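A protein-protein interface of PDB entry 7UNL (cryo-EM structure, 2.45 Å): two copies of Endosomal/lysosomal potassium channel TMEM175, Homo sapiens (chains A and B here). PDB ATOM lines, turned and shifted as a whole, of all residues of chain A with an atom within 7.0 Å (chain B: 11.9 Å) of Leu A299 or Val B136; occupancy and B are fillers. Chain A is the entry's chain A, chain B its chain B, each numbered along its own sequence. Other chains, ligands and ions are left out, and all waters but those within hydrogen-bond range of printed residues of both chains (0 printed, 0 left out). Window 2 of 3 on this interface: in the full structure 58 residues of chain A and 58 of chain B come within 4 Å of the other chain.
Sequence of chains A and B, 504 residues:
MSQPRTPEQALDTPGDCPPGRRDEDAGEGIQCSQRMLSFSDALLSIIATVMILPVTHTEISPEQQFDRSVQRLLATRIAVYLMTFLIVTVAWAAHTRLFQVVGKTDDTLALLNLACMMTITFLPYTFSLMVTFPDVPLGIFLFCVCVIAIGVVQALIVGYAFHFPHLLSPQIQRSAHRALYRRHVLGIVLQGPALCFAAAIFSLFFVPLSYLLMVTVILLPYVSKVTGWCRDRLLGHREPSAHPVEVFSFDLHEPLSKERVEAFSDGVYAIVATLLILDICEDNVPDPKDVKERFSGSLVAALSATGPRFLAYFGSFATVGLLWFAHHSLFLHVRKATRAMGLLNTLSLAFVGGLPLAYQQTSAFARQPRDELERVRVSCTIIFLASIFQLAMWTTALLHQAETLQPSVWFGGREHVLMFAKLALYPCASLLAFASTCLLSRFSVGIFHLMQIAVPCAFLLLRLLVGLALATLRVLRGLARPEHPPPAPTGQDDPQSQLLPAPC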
ATOM      1  N   PRO A 286      -4.795  13.627  12.902  1.00  0.00           N
ATOM      2  CA  PRO A 286      -5.866  13.797  11.910  1.00  0.00           C
ATOM      3  C   PRO A 286      -5.452  13.316  10.528  1.00  0.00           C
ATOM      4  O   PRO A 286      -4.316  13.514  10.093  1.00  0.00           O
ATOM      5  CB  PRO A 286      -6.127  15.308  11.919  1.00  0.00           C
ATOM      6  CG  PRO A 286      -5.596  15.795  13.202  1.00  0.00           C
ATOM      7  CD  PRO A 286      -4.472  14.892  13.585  1.00  0.00           C
ATOM      8  N   VAL A 291      -9.370  16.371   7.516  1.00  0.00           N
ATOM      9  CA  VAL A 291      -9.235  17.781   7.860  1.00  0.00           C
ATOM     10  C   VAL A 291      -9.888  18.629   6.776  1.00  0.00           C
ATOM     11  O   VAL A 291     -10.281  19.775   7.019  1.00  0.00           O
ATOM     12  CB  VAL A 291      -7.753  18.154   8.056  1.00  0.00           C
ATOM     13  CG1 VAL A 291      -7.494  19.619   7.718  1.00  0.00           C
ATOM     14  CG2 VAL A 291      -7.315  17.845   9.476  1.00  0.00           C
ATOM     15  N   PHE A 295     -13.809  18.971   8.463  1.00  0.00           N
ATOM     16  CA  PHE A 295     -13.367  20.102   9.270  1.00  0.00           C
ATOM     17  C   PHE A 295     -13.090  21.345   8.432  1.00  0.00           C
ATOM     18  O   PHE A 295     -12.534  22.316   8.961  1.00  0.00           O
ATOM     19  CB  PHE A 295     -12.122  19.722  10.077  1.00  0.00           C
ATOM     20  CG  PHE A 295     -12.412  18.811  11.234  1.00  0.00           C
ATOM     21  CD1 PHE A 295     -13.050  19.288  12.364  1.00  0.00           C
ATOM     22  CD2 PHE A 295     -12.053  17.476  11.188  1.00  0.00           C
ATOM     23  CE1 PHE A 295     -13.321  18.455  13.427  1.00  0.00           C
ATOM     24  CE2 PHE A 295     -12.319  16.638  12.249  1.00  0.00           C
ATOM     25  CZ  PHE A 295     -12.954  17.128  13.370  1.00  0.00           C
ATOM     26  N   SER A 296     -13.459  21.350   7.152  1.00  0.00           N
ATOM     27  CA  SER A 296     -13.358  22.541   6.308  1.00  0.00           C
ATOM     28  C   SER A 296     -11.924  23.057   6.224  1.00  0.00           C
ATOM     29  O   SER A 296     -11.686  24.265   6.146  1.00  0.00           O
ATOM     30  CB  SER A 296     -14.293  23.643   6.810  1.00  0.00           C
ATOM     31  OG  SER A 296     -14.421  24.677   5.851  1.00  0.00           O
ATOM     32  N   GLY A 297     -10.953  22.143   6.238  1.00  0.00           N
ATOM     33  CA  GLY A 297      -9.565  22.491   6.028  1.00  0.00           C
ATOM     34  C   GLY A 297      -8.840  23.039   7.238  1.00  0.00           C
ATOM     35  O   GLY A 297      -7.660  23.392   7.120  1.00  0.00           O
ATOM     36  N   SER A 298      -9.495  23.122   8.391  1.00  0.00           N
ATOM     37  CA  SER A 298      -8.889  23.695   9.585  1.00  0.00           C
ATOM     38  C   SER A 298      -8.262  22.590  10.427  1.00  0.00           C
ATOM     39  O   SER A 298      -8.975  21.763  11.007  1.00  0.00           O
ATOM     40  CB  SER A 298      -9.926  24.463  10.401  1.00  0.00           C
ATOM     41  OG  SER A 298      -9.364  24.950  11.607  1.00  0.00           O
ATOM     42  N   LEU A 299      -6.929  22.575  10.488  1.00  0.00           N
ATOM     43  CA  LEU A 299      -6.245  21.689  11.422  1.00  0.00           C
ATOM     44  C   LEU A 299      -6.520  22.096  12.863  1.00  0.00           C
ATOM     45  O   LEU A 299      -6.561  21.238  13.754  1.00  0.00           O
ATOM     46  CB  LEU A 299      -4.741  21.697  11.138  1.00  0.00           C
ATOM     47  CG  LEU A 299      -3.842  20.826  12.020  1.00  0.00           C
ATOM     48  CD1 LEU A 299      -4.281  19.376  11.995  1.00  0.00           C
ATOM     49  CD2 LEU A 299      -2.392  20.954  11.582  1.00  0.00           C
ATOM     50  N   VAL A 300      -6.723  23.393  13.103  1.00  0.00           N
ATOM     51  CA  VAL A 300      -7.030  23.873  14.448  1.00  0.00           C
ATOM     52  C   VAL A 300      -8.303  23.212  14.961  1.00  0.00           C
ATOM     53  O   VAL A 300      -8.346  22.689  16.080  1.00  0.00           O
ATOM     54  CB  VAL A 300      -7.153  25.408  14.447  1.00  0.00           C
ATOM     55  CG1 VAL A 300      -7.710  25.916  15.769  1.00  0.00           C
ATOM     56  CG2 VAL A 300      -5.807  26.048  14.151  1.00  0.00           C
ATOM     57  N   ALA A 301      -9.357  23.222  14.145  1.00  0.00           N
ATOM     58  CA  ALA A 301     -10.631  22.628  14.534  1.00  0.00           C
ATOM     59  C   ALA A 301     -10.553  21.117  14.705  1.00  0.00           C
ATOM     60  O   ALA A 301     -11.148  20.585  15.649  1.00  0.00           O
ATOM     61  CB  ALA A 301     -11.706  22.968  13.501  1.00  0.00           C
ATOM     62  N   ALA A 302      -9.841  20.417  13.825  1.00  0.00           N
ATOM     63  CA  ALA A 302      -9.676  18.978  13.970  1.00  0.00           C
ATOM     64  C   ALA A 302      -8.905  18.613  15.229  1.00  0.00           C
ATOM     65  O   ALA A 302      -9.221  17.603  15.868  1.00  0.00           O
ATOM     66  CB  ALA A 302      -8.966  18.401  12.743  1.00  0.00           C
ATOM     67  N   LEU A 303      -7.898  19.407  15.597  1.00  0.00           N
ATOM     68  CA  LEU A 303      -7.204  19.173  16.858  1.00  0.00           C
ATOM     69  C   LEU A 303      -8.104  19.487  18.046  1.00  0.00           C
ATOM     70  O   LEU A 303      -8.096  18.763  19.048  1.00  0.00           O
ATOM     71  CB  LEU A 303      -5.931  20.018  16.917  1.00  0.00           C
ATOM     72  CG  LEU A 303      -4.724  19.535  16.113  1.00  0.00           C
ATOM     73  CD1 LEU A 303      -3.571  20.487  16.342  1.00  0.00           C
ATOM     74  CD2 LEU A 303      -4.320  18.114  16.472  1.00  0.00           C
ATOM     75  N   SER A 304      -8.887  20.565  17.953  1.00  0.00           N
ATOM     76  CA  SER A 304      -9.776  20.936  19.048  1.00  0.00           C
ATOM     77  C   SER A 304     -10.851  19.884  19.274  1.00  0.00           C
ATOM     78  O   SER A 304     -11.301  19.690  20.409  1.00  0.00           O
ATOM     79  CB  SER A 304     -10.416  22.294  18.762  1.00  0.00           C
ATOM     80  OG  SER A 304      -9.483  23.342  18.948  1.00  0.00           O
ATOM     81  N   ALA A 305     -11.276  19.200  18.215  1.00  0.00           N
ATOM     82  CA  ALA A 305     -12.221  18.098  18.337  1.00  0.00           C
ATOM     83  C   ALA A 305     -11.617  16.879  19.030  1.00  0.00           C
ATOM     84  O   ALA A 305     -12.326  15.892  19.255  1.00  0.00           O
ATOM     85  CB  ALA A 305     -12.750  17.703  16.958  1.00  0.00           C
ATOM     86  N   TYR B 125       3.968  12.919  19.103  1.00  0.00           N
ATOM     87  CA  TYR B 125       2.734  13.372  18.475  1.00  0.00           C
ATOM     88  C   TYR B 125       2.963  14.641  17.665  1.00  0.00           C
ATOM     89  O   TYR B 125       2.475  14.760  16.535  1.00  0.00           O
ATOM     90  CB  TYR B 125       1.661  13.599  19.540  1.00  0.00           C
ATOM     91  CG  TYR B 125       0.336  14.065  18.987  1.00  0.00           C
ATOM     92  CD1 TYR B 125       0.054  15.415  18.850  1.00  0.00           C
ATOM     93  CD2 TYR B 125      -0.631  13.152  18.598  1.00  0.00           C
ATOM     94  CE1 TYR B 125      -1.151  15.841  18.343  1.00  0.00           C
ATOM     95  CE2 TYR B 125      -1.840  13.571  18.091  1.00  0.00           C
ATOM     96  CZ  TYR B 125      -2.096  14.915  17.965  1.00  0.00           C
ATOM     97  OH  TYR B 125      -3.300  15.337  17.459  1.00  0.00           O
ATOM     98  N   THR B 126       3.706  15.596  18.223  1.00  0.00           N
ATOM     99  CA  THR B 126       3.939  16.853  17.522  1.00  0.00           C
ATOM    100  C   THR B 126       4.792  16.648  16.276  1.00  0.00           C
ATOM    101  O   THR B 126       4.526  17.257  15.235  1.00  0.00           O
ATOM    102  CB  THR B 126       4.588  17.869  18.461  1.00  0.00           C
ATOM    103  OG1 THR B 126       5.749  17.296  19.075  1.00  0.00           O
ATOM    104  CG2 THR B 126       3.609  18.295  19.535  1.00  0.00           C
ATOM    105  N   PHE B 127       5.822  15.802  16.356  1.00  0.00           N
ATOM    106  CA  PHE B 127       6.630  15.529  15.170  1.00  0.00           C
ATOM    107  C   PHE B 127       5.810  14.816  14.099  1.00  0.00           C
ATOM    108  O   PHE B 127       5.918  15.137  12.907  1.00  0.00           O
ATOM    109  CB  PHE B 127       7.860  14.703  15.543  1.00  0.00           C
ATOM    110  CG  PHE B 127       8.728  14.354  14.372  1.00  0.00           C
ATOM    111  CD1 PHE B 127       9.689  15.242  13.922  1.00  0.00           C
ATOM    112  CD2 PHE B 127       8.585  13.144  13.717  1.00  0.00           C
ATOM    113  CE1 PHE B 127      10.487  14.930  12.845  1.00  0.00           C
ATOM    114  CE2 PHE B 127       9.382  12.828  12.640  1.00  0.00           C
ATOM    115  CZ  PHE B 127      10.333  13.723  12.203  1.00  0.00           C
ATOM    116  N   SER B 128       4.988  13.842  14.502  1.00  0.00           N
ATOM    117  CA  SER B 128       4.120  13.152  13.559  1.00  0.00           C
ATOM    118  C   SER B 128       3.148  14.105  12.884  1.00  0.00           C
ATOM    119  O   SER B 128       2.927  13.998  11.674  1.00  0.00           O
ATOM    120  CB  SER B 128       3.346  12.046  14.274  1.00  0.00           C
ATOM    121  OG  SER B 128       2.733  11.164  13.351  1.00  0.00           O
ATOM    122  N   LEU B 129       2.565  15.032  13.639  1.00  0.00           N
ATOM    123  CA  LEU B 129       1.696  16.056  13.081  1.00  0.00           C
ATOM    124  C   LEU B 129       2.429  17.013  12.154  1.00  0.00           C
ATOM    125  O   LEU B 129       1.871  17.415  11.128  1.00  0.00           O
ATOM    126  CB  LEU B 129       1.045  16.849  14.218  1.00  0.00           C
ATOM    127  CG  LEU B 129      -0.209  17.644  13.876  1.00  0.00           C
ATOM    128  CD1 LEU B 129      -1.360  16.707  13.574  1.00  0.00           C
ATOM    129  CD2 LEU B 129      -0.556  18.565  15.020  1.00  0.00           C
ATOM    130  N   MET B 130       3.662  17.386  12.497  1.00  0.00           N
ATOM    131  CA  MET B 130       4.454  18.245  11.626  1.00  0.00           C
ATOM    132  C   MET B 130       4.729  17.570  10.289  1.00  0.00           C
ATOM    133  O   MET B 130       4.621  18.203   9.232  1.00  0.00           O
ATOM    134  CB  MET B 130       5.766  18.610  12.321  1.00  0.00           C
ATOM    135  CG  MET B 130       6.631  19.596  11.563  1.00  0.00           C
ATOM    136  SD  MET B 130       8.091  20.113  12.490  1.00  0.00           S
ATOM    137  CE  MET B 130       8.895  18.544  12.789  1.00  0.00           C
ATOM    138  N   VAL B 131       5.088  16.286  10.315  1.00  0.00           N
ATOM    139  CA  VAL B 131       5.364  15.582   9.064  1.00  0.00           C
ATOM    140  C   VAL B 131       4.075  15.312   8.296  1.00  0.00           C
ATOM    141  O   VAL B 131       4.079  15.254   7.062  1.00  0.00           O
ATOM    142  CB  VAL B 131       6.146  14.280   9.326  1.00  0.00           C
ATOM    143  CG1 VAL B 131       7.535  14.592   9.861  1.00  0.00           C
ATOM    144  CG2 VAL B 131       5.389  13.365  10.263  1.00  0.00           C
ATOM    145  N   THR B 132       2.957  15.129   9.004  1.00  0.00           N
ATOM    146  CA  THR B 132       1.698  14.831   8.329  1.00  0.00           C
ATOM    147  C   THR B 132       1.102  16.066   7.661  1.00  0.00           C
ATOM    148  O   THR B 132       0.386  15.940   6.662  1.00  0.00           O
ATOM    149  CB  THR B 132       0.700  14.233   9.320  1.00  0.00           C
ATOM    150  OG1 THR B 132       1.302  13.130  10.008  1.00  0.00           O
ATOM    151  CG2 THR B 132      -0.547  13.752   8.599  1.00  0.00           C
ATOM    152  N   PHE B 133       1.383  17.258   8.189  1.00  0.00           N
ATOM    153  CA  PHE B 133       0.869  18.517   7.651  1.00  0.00           C
ATOM    154  C   PHE B 133       2.037  19.466   7.408  1.00  0.00           C
ATOM    155  O   PHE B 133       2.207  20.462   8.125  1.00  0.00           O
ATOM    156  CB  PHE B 133      -0.154  19.146   8.594  1.00  0.00           C
ATOM    157  CG  PHE B 133      -1.456  18.407   8.653  1.00  0.00           C
ATOM    158  CD1 PHE B 133      -1.644  17.376   9.555  1.00  0.00           C
ATOM    159  CD2 PHE B 133      -2.492  18.742   7.802  1.00  0.00           C
ATOM    160  CE1 PHE B 133      -2.838  16.698   9.608  1.00  0.00           C
ATOM    161  CE2 PHE B 133      -3.689  18.067   7.850  1.00  0.00           C
ATOM    162  CZ  PHE B 133      -3.863  17.043   8.754  1.00  0.00           C
ATOM    163  N   PRO B 134       2.864  19.184   6.400  1.00  0.00           N
ATOM    164  CA  PRO B 134       4.036  20.036   6.149  1.00  0.00           C
ATOM    165  C   PRO B 134       3.705  21.495   5.883  1.00  0.00           C
ATOM    166  O   PRO B 134       4.461  22.371   6.319  1.00  0.00           O
ATOM    167  CB  PRO B 134       4.676  19.379   4.914  1.00  0.00           C
ATOM    168  CG  PRO B 134       3.593  18.453   4.377  1.00  0.00           C
ATOM    169  CD  PRO B 134       2.956  17.951   5.610  1.00  0.00           C
ATOM    170  N   ASP B 135       2.610  21.789   5.184  1.00  0.00           N
ATOM    171  CA  ASP B 135       2.306  23.147   4.754  1.00  0.00           C
ATOM    172  C   ASP B 135       1.510  23.942   5.779  1.00  0.00           C
ATOM    173  O   ASP B 135       1.255  25.130   5.557  1.00  0.00           O
ATOM    174  CB  ASP B 135       1.543  23.116   3.426  1.00  0.00           C
ATOM    175  CG  ASP B 135       2.134  22.131   2.439  1.00  0.00           C
ATOM    176  OD1 ASP B 135       3.377  22.060   2.341  1.00  0.00           O
ATOM    177  OD2 ASP B 135       1.356  21.429   1.760  1.00  0.00           O
ATOM    178  N   VAL B 136       1.110  23.330   6.889  1.00  0.00           N
ATOM    179  CA  VAL B 136       0.393  24.022   7.952  1.00  0.00           C
ATOM    180  C   VAL B 136       1.428  24.512   8.966  1.00  0.00           C
ATOM    181  O   VAL B 136       2.135  23.679   9.552  1.00  0.00           O
ATOM    182  CB  VAL B 136      -0.644  23.114   8.620  1.00  0.00           C
ATOM    183  CG1 VAL B 136      -1.479  23.903   9.616  1.00  0.00           C
ATOM    184  CG2 VAL B 136      -1.537  22.470   7.573  1.00  0.00           C
ATOM    185  N   PRO B 137       1.549  25.822   9.195  1.00  0.00           N
ATOM    186  CA  PRO B 137       2.588  26.304  10.116  1.00  0.00           C
ATOM    187  C   PRO B 137       2.346  25.919  11.563  1.00  0.00           C
ATOM    188  O   PRO B 137       3.251  26.088  12.388  1.00  0.00           O
ATOM    189  CB  PRO B 137       2.537  27.824   9.925  1.00  0.00           C
ATOM    190  CG  PRO B 137       1.118  28.085   9.595  1.00  0.00           C
ATOM    191  CD  PRO B 137       0.691  26.926   8.730  1.00  0.00           C
ATOM    192  N   LEU B 138       1.156  25.421  11.901  1.00  0.00           N
ATOM    193  CA  LEU B 138       0.851  25.129  13.296  1.00  0.00           C
ATOM    194  C   LEU B 138       1.615  23.910  13.802  1.00  0.00           C
ATOM    195  O   LEU B 138       1.932  23.834  14.993  1.00  0.00           O
ATOM    196  CB  LEU B 138      -0.657  24.931  13.463  1.00  0.00           C
ATOM    197  CG  LEU B 138      -1.176  24.417  14.809  1.00  0.00           C
ATOM    198  CD1 LEU B 138      -1.607  25.573  15.686  1.00  0.00           C
ATOM    199  CD2 LEU B 138      -2.328  23.458  14.601  1.00  0.00           C
ATOM    200  N   GLY B 139       1.909  22.944  12.931  1.00  0.00           N
ATOM    201  CA  GLY B 139       2.615  21.754  13.382  1.00  0.00           C
ATOM    202  C   GLY B 139       4.024  22.051  13.862  1.00  0.00           C
ATOM    203  O   GLY B 139       4.438  21.590  14.935  1.00  0.00           O
ATOM    204  N   ILE B 140       4.779  22.828  13.083  1.00  0.00           N
ATOM    205  CA  ILE B 140       6.121  23.208  13.504  1.00  0.00           C
ATOM    206  C   ILE B 140       6.049  24.056  14.765  1.00  0.00           C
ATOM    207  O   ILE B 140       6.904  23.950  15.651  1.00  0.00           O
ATOM    208  CB  ILE B 140       6.874  23.932  12.366  1.00  0.00           C
ATOM    209  CG1 ILE B 140       6.358  25.359  12.169  1.00  0.00           C
ATOM    210  CG2 ILE B 140       6.768  23.167  11.054  1.00  0.00           C
ATOM    211  CD1 ILE B 140       7.236  26.416  12.788  1.00  0.00           C
ATOM    212  N   PHE B 141       5.019  24.897  14.873  1.00  0.00           N
ATOM    213  CA  PHE B 141       4.836  25.712  16.067  1.00  0.00           C
ATOM    214  C   PHE B 141       4.644  24.838  17.298  1.00  0.00           C
ATOM    215  O   PHE B 141       5.264  25.067  18.341  1.00  0.00           O
ATOM    216  CB  PHE B 141       3.643  26.648  15.863  1.00  0.00           C
ATOM    217  CG  PHE B 141       3.048  27.170  17.139  1.00  0.00           C
ATOM    218  CD1 PHE B 141       3.608  28.254  17.791  1.00  0.00           C
ATOM    219  CD2 PHE B 141       1.915  26.584  17.678  1.00  0.00           C
ATOM    220  CE1 PHE B 141       3.056  28.736  18.961  1.00  0.00           C
ATOM    221  CE2 PHE B 141       1.360  27.061  18.846  1.00  0.00           C
ATOM    222  CZ  PHE B 141       1.930  28.138  19.488  1.00  0.00           C
ATOM    223  N   LEU B 142       3.790  23.818  17.190  1.00  0.00           N
ATOM    224  CA  LEU B 142       3.551  22.925  18.318  1.00  0.00           C
ATOM    225  C   LEU B 142       4.818  22.168  18.702  1.00  0.00           C
ATOM    226  O   LEU B 142       5.146  22.048  19.890  1.00  0.00           O
ATOM    227  CB  LEU B 142       2.430  21.942  17.976  1.00  0.00           C
ATOM    228  CG  LEU B 142       1.016  22.508  17.832  1.00  0.00           C
ATOM    229  CD1 LEU B 142       0.049  21.410  17.426  1.00  0.00           C
ATOM    230  CD2 LEU B 142       0.553  23.169  19.113  1.00  0.00           C
ATOM    231  N   PHE B 143       5.543  21.647  17.709  1.00  0.00           N
ATOM    232  CA  PHE B 143       6.764  20.903  18.004  1.00  0.00           C
ATOM    233  C   PHE B 143       7.798  21.795  18.687  1.00  0.00           C
ATOM    234  O   PHE B 143       8.400  21.417  19.704  1.00  0.00           O
ATOM    235  CB  PHE B 143       7.322  20.305  16.710  1.00  0.00           C
ATOM    236  CG  PHE B 143       8.630  19.596  16.882  1.00  0.00           C
ATOM    237  CD1 PHE B 143       8.673  18.329  17.431  1.00  0.00           C
ATOM    238  CD2 PHE B 143       9.817  20.188  16.487  1.00  0.00           C
ATOM    239  CE1 PHE B 143       9.869  17.669  17.591  1.00  0.00           C
ATOM    240  CE2 PHE B 143      11.017  19.530  16.644  1.00  0.00           C
ATOM    241  CZ  PHE B 143      11.043  18.268  17.197  1.00  0.00           C
ATOM    242  N   CYS B 144       8.000  23.001  18.149  1.00  0.00           N
ATOM    243  CA  CYS B 144       8.958  23.930  18.733  1.00  0.00           C
ATOM    244  C   CYS B 144       8.539  24.341  20.136  1.00  0.00           C
ATOM    245  O   CYS B 144       9.386  24.510  21.019  1.00  0.00           O
ATOM    246  CB  CYS B 144       9.102  25.156  17.834  1.00  0.00           C
ATOM    247  SG  CYS B 144      10.003  24.852  16.301  1.00  0.00           S
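Printed residues of chain B that touch a printed residue of chain A: Tyr B125, Leu B129, Phe B133, Val B136, Leu B138 and Leu B142.
Hydrophobic or aromatic side chains of chain B that line the printed part of chain A: Tyr B125, Leu B129, Phe B133, Val B136, Leu B138 and Leu B142.
Along chain B the printed residues that touch a printed residue of chain A span positions 125 to 142.
Of the 13 printed residues of chain A, 4 touch a printed residue of chain B.
Printed residues of chain A that touch a printed residue of chain B: Pro A286, Val A291, Leu A299 and Leu A303.
Among the printed residues, 10 pairs touch across the chains.
Among the printed residues, no Asp or Glu carboxylate lies within 4 Å of a Lys or Arg side-chain nitrogen of the other chain.
No position is printed for both chains.
Of the 10 pairs that touch across the chains among the printed residues, none has its exchanged pair printed and touching as well.
Leu A299 touches just these residues of chain B: Phe B133, Val B136 and Leu B138.
Val B136 touches one residue of chain A.
Pro A286 touches two residues of chain B.
Val A291 touches just one residue of chain B: Phe B133.
No residue of chain B comes within 4 Å of Gly A297.
No residue of chain B comes within 4 Å of Ser A298.
No residue of chain B comes within 4 Å of Val A300.
Ala A302 touches none of the printed residues of chain B.
Leu A303 touches four residues of chain B.
Of the printed residues of chain A, Leu B138 touches Leu A299 and Leu A303.
Printed residues of chain A within 4 Å of Leu B142: Leu A303 (3.9 Å).
Printed residues of chain A within 4 Å of Leu B129: Pro A286 (3.6 Å) and Leu A303 (3.8 Å).
The nearest residue of chain A that does not touch Val B136 is Gly A297 (6.2 Å).
The nearest printed residue of chain A that does not touch Leu B129 is Leu A299 (4.3 Å).
Leu B129 touches Pro A286.
Pro A286 touches Phe B133 (O to CE1, 3.5 Å).
CG2 of Val A291 touches CZ of Phe B133, 3.6 Å away.
Phe B133 touches Leu A299 (CE1 to CD1, 3.9 Å).
Leu A299 touches Val B136 (CD2 to CG1, 3.7 Å).
CD2 of Leu B138 touches CD2 of Leu A299, at 3.9 Å.
Leu A303 touches Tyr B125.
Leu A303 touches Leu B129.
Leu A303 touches Leu B138.
Leu B142 touches Leu A303 (CD1 to CD1, 3.9 Å).
O of Val A291 sits at hydrogen-bond distance from N of Gly A297, 2.6 Å away.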
